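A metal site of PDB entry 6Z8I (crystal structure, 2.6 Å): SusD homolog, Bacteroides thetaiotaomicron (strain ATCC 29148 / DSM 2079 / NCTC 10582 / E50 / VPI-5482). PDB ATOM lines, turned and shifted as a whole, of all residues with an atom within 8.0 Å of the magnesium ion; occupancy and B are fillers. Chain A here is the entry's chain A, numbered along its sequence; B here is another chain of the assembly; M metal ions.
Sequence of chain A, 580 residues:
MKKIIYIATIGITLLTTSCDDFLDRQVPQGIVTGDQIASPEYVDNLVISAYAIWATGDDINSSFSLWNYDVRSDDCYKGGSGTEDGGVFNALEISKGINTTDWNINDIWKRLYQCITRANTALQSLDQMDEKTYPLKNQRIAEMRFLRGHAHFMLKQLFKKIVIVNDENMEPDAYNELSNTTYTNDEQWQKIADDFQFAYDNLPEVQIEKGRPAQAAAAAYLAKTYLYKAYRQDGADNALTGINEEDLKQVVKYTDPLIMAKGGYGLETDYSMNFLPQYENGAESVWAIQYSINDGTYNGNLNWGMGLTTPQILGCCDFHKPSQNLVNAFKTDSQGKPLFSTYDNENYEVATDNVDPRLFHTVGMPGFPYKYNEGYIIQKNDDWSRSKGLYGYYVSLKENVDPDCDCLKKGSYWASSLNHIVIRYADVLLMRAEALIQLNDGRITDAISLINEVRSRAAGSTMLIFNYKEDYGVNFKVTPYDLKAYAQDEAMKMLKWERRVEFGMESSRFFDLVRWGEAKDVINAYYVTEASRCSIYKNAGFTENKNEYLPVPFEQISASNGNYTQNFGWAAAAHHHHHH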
ATOM      1  N   PRO A 277     -21.854   4.505 -15.979  1.00  0.00           N
ATOM      2  CA  PRO A 277     -22.928   3.968 -15.105  1.00  0.00           C
ATOM      3  C   PRO A 277     -22.774   2.504 -14.760  1.00  0.00           C
ATOM      4  O   PRO A 277     -23.025   2.105 -13.605  1.00  0.00           O
ATOM      5  CB  PRO A 277     -24.194   4.199 -15.936  1.00  0.00           C
ATOM      6  CG  PRO A 277     -23.828   5.275 -16.922  1.00  0.00           C
ATOM      7  CD  PRO A 277     -22.382   5.057 -17.236  1.00  0.00           C
ATOM      8  N   GLU A 280     -20.305   1.962 -11.284  1.00  0.00           N
ATOM      9  CA  GLU A 280     -20.351   2.761 -10.073  1.00  0.00           C
ATOM     10  C   GLU A 280     -19.784   1.975  -8.887  1.00  0.00           C
ATOM     11  O   GLU A 280     -19.797   0.753  -8.864  1.00  0.00           O
ATOM     12  CB  GLU A 280     -21.780   3.198  -9.794  1.00  0.00           C
ATOM     13  CG  GLU A 280     -22.282   4.317 -10.708  1.00  0.00           C
ATOM     14  CD  GLU A 280     -23.669   4.739 -10.343  1.00  0.00           C
ATOM     15  OE1 GLU A 280     -24.333   3.965  -9.622  1.00  0.00           O
ATOM     16  OE2 GLU A 280     -24.114   5.827 -10.787  1.00  0.00           O
ATOM     17  N   ASN A 281     -19.236   2.715  -7.923  1.00  0.00           N
ATOM     18  CA  ASN A 281     -18.783   2.137  -6.653  1.00  0.00           C
ATOM     19  C   ASN A 281     -17.725   1.054  -6.838  1.00  0.00           C
ATOM     20  O   ASN A 281     -17.687   0.059  -6.114  1.00  0.00           O
ATOM     21  CB  ASN A 281     -19.988   1.624  -5.845  1.00  0.00           C
ATOM     22  CG  ASN A 281     -20.957   2.770  -5.475  1.00  0.00           C
ATOM     23  OD1 ASN A 281     -20.581   3.941  -5.516  1.00  0.00           O
ATOM     24  ND2 ASN A 281     -22.181   2.426  -5.170  1.00  0.00           N
ATOM     25  N   ALA A 288     -18.385   8.896  -3.023  1.00  0.00           N
ATOM     26  CA  ALA A 288     -19.105   9.433  -4.153  1.00  0.00           C
ATOM     27  C   ALA A 288     -20.527   9.831  -3.764  1.00  0.00           C
ATOM     28  O   ALA A 288     -21.070   9.361  -2.752  1.00  0.00           O
ATOM     29  CB  ALA A 288     -19.170   8.435  -5.315  1.00  0.00           C
ATOM     30  N   ILE A 289     -21.123  10.703  -4.570  1.00  0.00           N
ATOM     31  CA  ILE A 289     -22.487  11.150  -4.366  1.00  0.00           C
ATOM     32  C   ILE A 289     -23.385  10.221  -5.174  1.00  0.00           C
ATOM     33  O   ILE A 289     -23.249  10.134  -6.395  1.00  0.00           O
ATOM     34  CB  ILE A 289     -22.688  12.607  -4.801  1.00  0.00           C
ATOM     35  CG1 ILE A 289     -21.719  13.513  -4.052  1.00  0.00           C
ATOM     36  CG2 ILE A 289     -24.122  13.029  -4.557  1.00  0.00           C
ATOM     37  CD1 ILE A 289     -21.672  13.304  -2.553  1.00  0.00           C
ATOM     38  N   GLN A 290     -24.314   9.553  -4.485  1.00  0.00           N
ATOM     39  CA  GLN A 290     -25.123   8.470  -5.054  1.00  0.00           C
ATOM     40  C   GLN A 290     -26.391   8.987  -5.746  1.00  0.00           C
ATOM     41  O   GLN A 290     -27.516   8.756  -5.306  1.00  0.00           O
ATOM     42  CB  GLN A 290     -25.471   7.465  -3.968  1.00  0.00           C
ATOM     43  CG  GLN A 290     -24.281   6.958  -3.215  1.00  0.00           C
ATOM     44  CD  GLN A 290     -23.506   5.941  -4.037  1.00  0.00           C
ATOM     45  OE1 GLN A 290     -24.086   5.143  -4.777  1.00  0.00           O
ATOM     46  NE2 GLN A 290     -22.184   5.981  -3.918  1.00  0.00           N
ATOM     47  N   TYR A 291     -26.207   9.662  -6.869  1.00  0.00           N
ATOM     48  CA  TYR A 291     -27.311   9.986  -7.746  1.00  0.00           C
ATOM     49  C   TYR A 291     -28.044   8.718  -8.173  1.00  0.00           C
ATOM     50  O   TYR A 291     -27.414   7.693  -8.449  1.00  0.00           O
ATOM     51  CB  TYR A 291     -26.780  10.755  -8.967  1.00  0.00           C
ATOM     52  CG  TYR A 291     -26.202  12.109  -8.582  1.00  0.00           C
ATOM     53  CD1 TYR A 291     -24.829  12.362  -8.616  1.00  0.00           C
ATOM     54  CD2 TYR A 291     -27.048  13.149  -8.153  1.00  0.00           C
ATOM     55  CE1 TYR A 291     -24.309  13.614  -8.238  1.00  0.00           C
ATOM     56  CE2 TYR A 291     -26.533  14.382  -7.802  1.00  0.00           C
ATOM     57  CZ  TYR A 291     -25.159  14.618  -7.835  1.00  0.00           C
ATOM     58  OH  TYR A 291     -24.673  15.869  -7.442  1.00  0.00           O
ATOM     59  N   SER A 292     -29.367   8.792  -8.242  1.00  0.00           N
ATOM     60  CA  SER A 292     -30.188   7.604  -8.443  1.00  0.00           C
ATOM     61  C   SER A 292     -31.423   7.904  -9.294  1.00  0.00           C
ATOM     62  O   SER A 292     -31.795   9.062  -9.527  1.00  0.00           O
ATOM     63  CB  SER A 292     -30.593   7.006  -7.090  1.00  0.00           C
ATOM     64  OG  SER A 292     -31.561   7.817  -6.440  1.00  0.00           O
ATOM     65  N   ILE A 293     -32.059   6.832  -9.752  1.00  0.00           N
ATOM     66  CA  ILE A 293     -33.154   6.878 -10.711  1.00  0.00           C
ATOM     67  C   ILE A 293     -34.147   5.773 -10.375  1.00  0.00           C
ATOM     68  O   ILE A 293     -33.822   4.785  -9.699  1.00  0.00           O
ATOM     69  CB  ILE A 293     -32.644   6.762 -12.166  1.00  0.00           C
ATOM     70  CG1 ILE A 293     -33.702   7.213 -13.180  1.00  0.00           C
ATOM     71  CG2 ILE A 293     -32.105   5.308 -12.453  1.00  0.00           C
ATOM     72  CD1 ILE A 293     -33.189   7.098 -14.620  1.00  0.00           C
ATOM     73  N   ASN A 301     -33.379  11.203  -8.372  1.00  0.00           N
ATOM     74  CA  ASN A 301     -32.300  11.995  -7.794  1.00  0.00           C
ATOM     75  C   ASN A 301     -31.137  12.002  -8.787  1.00  0.00           C
ATOM     76  O   ASN A 301     -30.062  11.433  -8.555  1.00  0.00           O
ATOM     77  CB  ASN A 301     -31.853  11.457  -6.437  1.00  0.00           C
ATOM     78  CG  ASN A 301     -32.658  12.006  -5.296  1.00  0.00           C
ATOM     79  OD1 ASN A 301     -33.460  12.948  -5.446  1.00  0.00           O
ATOM     80  ND2 ASN A 301     -32.454  11.426  -4.112  1.00  0.00           N
ATOM     81  N   LEU A 302     -31.377  12.642  -9.916  1.00  0.00           N
ATOM     82  CA  LEU A 302     -30.319  12.742 -10.898  1.00  0.00           C
ATOM     83  C   LEU A 302     -29.409  13.920 -10.571  1.00  0.00           C
ATOM     84  O   LEU A 302     -29.686  14.754  -9.687  1.00  0.00           O
ATOM     85  CB  LEU A 302     -30.876  12.858 -12.326  1.00  0.00           C
ATOM     86  CG  LEU A 302     -31.999  11.854 -12.652  1.00  0.00           C
ATOM     87  CD1 LEU A 302     -32.558  12.118 -14.033  1.00  0.00           C
ATOM     88  CD2 LEU A 302     -31.592  10.351 -12.503  1.00  0.00           C
ATOM     89  N   CYS A 407     -30.098   5.451 -17.806  1.00  0.00           N
ATOM     90  CA  CYS A 407     -29.832   6.370 -16.708  1.00  0.00           C
ATOM     91  C   CYS A 407     -30.080   7.823 -17.059  1.00  0.00           C
ATOM     92  O   CYS A 407     -30.010   8.670 -16.179  1.00  0.00           O
ATOM     93  CB  CYS A 407     -28.381   6.182 -16.268  1.00  0.00           C
ATOM     94  SG  CYS A 407     -27.210   6.639 -17.574  1.00  0.00           S
ATOM     95  N   SER A 416     -28.517  12.567 -15.325  1.00  0.00           N
ATOM     96  CA  SER A 416     -28.252  11.135 -15.213  1.00  0.00           C
ATOM     97  C   SER A 416     -28.019  10.724 -13.764  1.00  0.00           C
ATOM     98  O   SER A 416     -27.815  11.556 -12.885  1.00  0.00           O
ATOM     99  CB  SER A 416     -27.024  10.716 -16.043  1.00  0.00           C
ATOM    100  OG  SER A 416     -25.848  10.727 -15.246  1.00  0.00           O
ATOM    101  N   SER A 417     -28.014   9.395 -13.525  1.00  0.00           N
ATOM    102  CA  SER A 417     -27.815   8.818 -12.194  1.00  0.00           C
ATOM    103  C   SER A 417     -26.350   8.490 -11.892  1.00  0.00           C
ATOM    104  O   SER A 417     -26.062   7.806 -10.866  1.00  0.00           O
ATOM    105  CB  SER A 417     -28.642   7.542 -12.052  1.00  0.00           C
ATOM    106  OG  SER A 417     -28.038   6.497 -12.787  1.00  0.00           O
ATOM    107  N   LEU A 418     -25.462   8.934 -12.787  1.00  0.00           N
ATOM    108  CA  LEU A 418     -24.033   8.684 -12.687  1.00  0.00           C
ATOM    109  C   LEU A 418     -23.498   9.298 -11.419  1.00  0.00           C
ATOM    110  O   LEU A 418     -23.593  10.515 -11.227  1.00  0.00           O
ATOM    111  CB  LEU A 418     -23.316   9.290 -13.896  1.00  0.00           C
ATOM    112  CG  LEU A 418     -21.788   9.176 -14.012  1.00  0.00           C
ATOM    113  CD1 LEU A 418     -21.306   7.711 -14.052  1.00  0.00           C
ATOM    114  CD2 LEU A 418     -21.314   9.953 -15.242  1.00  0.00           C
ATOM    115  N   ASN A 419     -22.964   8.443 -10.555  1.00  0.00           N
ATOM    116  CA  ASN A 419     -22.353   8.904  -9.307  1.00  0.00           C
ATOM    117  C   ASN A 419     -21.281   9.953  -9.600  1.00  0.00           C
ATOM    118  O   ASN A 419     -20.597   9.885 -10.626  1.00  0.00           O
ATOM    119  CB  ASN A 419     -21.751   7.722  -8.544  1.00  0.00           C
ATOM    120  CG  ASN A 419     -22.804   6.850  -7.861  1.00  0.00           C
ATOM    121  OD1 ASN A 419     -23.998   6.927  -8.165  1.00  0.00           O
ATOM    122  ND2 ASN A 419     -22.352   6.006  -6.949  1.00  0.00           N
ATOM    123  N   HIS A 420     -21.165  10.947  -8.734  1.00  0.00           N
ATOM    124  CA  HIS A 420     -20.089  11.905  -8.817  1.00  0.00           C
ATOM    125  C   HIS A 420     -19.032  11.555  -7.774  1.00  0.00           C
ATOM    126  O   HIS A 420     -19.317  11.534  -6.575  1.00  0.00           O
ATOM    127  CB  HIS A 420     -20.585  13.321  -8.617  1.00  0.00           C
ATOM    128  CG  HIS A 420     -19.502  14.336  -8.735  1.00  0.00           C
ATOM    129  ND1 HIS A 420     -18.935  14.953  -7.628  1.00  0.00           N
ATOM    130  CD2 HIS A 420     -18.844  14.814  -9.811  1.00  0.00           C
ATOM    131  CE1 HIS A 420     -17.991  15.785  -8.034  1.00  0.00           C
ATOM    132  NE2 HIS A 420     -17.908  15.717  -9.353  1.00  0.00           N
ATOM    133  N   ASP B 684     -29.994   7.581  -1.934  1.00  0.00           N
ATOM    134  CA  ASP B 684     -29.512   6.244  -2.231  1.00  0.00           C
ATOM    135  C   ASP B 684     -28.354   5.815  -1.337  1.00  0.00           C
ATOM    136  O   ASP B 684     -27.249   5.537  -1.835  1.00  0.00           O
ATOM    137  CB  ASP B 684     -29.099   6.169  -3.694  1.00  0.00           C
ATOM    138  CG  ASP B 684     -28.779   4.774  -4.131  1.00  0.00           C
ATOM    139  OD1 ASP B 684     -28.007   4.644  -5.114  1.00  0.00           O
ATOM    140  OD2 ASP B 684     -29.287   3.819  -3.491  1.00  0.00           O
ATOM    141  N   GLY B 687     -26.259   2.718  -2.483  1.00  0.00           N
ATOM    142  CA  GLY B 687     -25.554   2.641  -3.754  1.00  0.00           C
ATOM    143  C   GLY B 687     -26.256   1.823  -4.807  1.00  0.00           C
ATOM    144  O   GLY B 687     -25.750   1.694  -5.916  1.00  0.00           O
ATOM    145  N   SER B 688     -27.412   1.242  -4.471  1.00  0.00           N
ATOM    146  CA  SER B 688     -28.312   0.560  -5.385  1.00  0.00           C
ATOM    147  C   SER B 688     -28.384   1.194  -6.758  1.00  0.00           C
ATOM    148  O   SER B 688     -28.351   0.505  -7.777  1.00  0.00           O
ATOM    149  CB  SER B 688     -29.713   0.557  -4.765  1.00  0.00           C
ATOM    150  OG  SER B 688     -30.272   1.860  -4.826  1.00  0.00           O
ATOM    151  N   ASN B 689     -28.554   2.509  -6.789  1.00  0.00           N
ATOM    152  CA  ASN B 689     -28.826   3.413  -7.923  1.00  0.00           C
ATOM    153  C   ASN B 689     -30.329   3.569  -8.079  1.00  0.00           C
ATOM    154  O   ASN B 689     -30.765   4.183  -9.064  1.00  0.00           O
ATOM    155  CB  ASN B 689     -28.182   2.988  -9.254  1.00  0.00           C
ATOM    156  CG  ASN B 689     -27.909   4.174 -10.154  1.00  0.00           C
ATOM    157  OD1 ASN B 689     -27.292   5.196  -9.746  1.00  0.00           O
ATOM    158  ND2 ASN B 689     -28.349   4.052 -11.417  1.00  0.00           N
ATOM    159  N   GLY B 690     -31.139   3.019  -7.172  1.00  0.00           N
ATOM    160  CA  GLY B 690     -32.559   3.319  -7.140  1.00  0.00           C
ATOM    161  C   GLY B 690     -33.409   2.070  -7.279  1.00  0.00           C
ATOM    162  O   GLY B 690     -33.150   1.043  -6.620  1.00  0.00           O
HETATM  163 MG    MG M   1     -25.882   6.266  -8.903  1.00  0.00          MG
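The side-chain carboxylate of Asp 684 of chain B is in hydrogen-bond range of the backbone NH of Asn 689 of chain B, at 2.8 Å. N of Ser 417 sits at hydrogen-bond distance from O of Cys 407 (3.4 Å). ND2 of Asn 419 lies within hydrogen-bond range of OE1 of Gln 290 (2.9 Å). OE1 of Glu 280 lies close to OD1 of Asn 689 of chain B, at 3.2 Å. The side-chain carboxylate (OE2) of Glu 280 is in hydrogen-bond range of the backbone NH (N) of Asn 419 (2.9 Å). The backbone NH (N) of Ile 293 lies within hydrogen-bond range of the backbone carbonyl oxygen (O) of Asn 689 of chain B (3.0 Å). OD1 of Asn 281 is in hydrogen-bond range of ND2 of Asn 419 (3.1 Å).
Along chain A the residues within 4 Å of the magnesium ion span positions 280 to 419.
The magnesium ion is bound by the side-chain amide oxygen (OD1) of Asn 689 of chain B (2.0 Å), the side-chain amide oxygen (OD1) of Asn 419 (2.1 Å), the backbone carbonyl oxygen (O) of Tyr 291 (2.1 Å) and the backbone carbonyl oxygen (O) of Ser 417 (2.5 Å). The magnesium ion has four donor atoms within binding distance. Slightly farther from the magnesium ion lies the side-chain carboxylate (OE2) of Glu 280 (2.6 Å).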
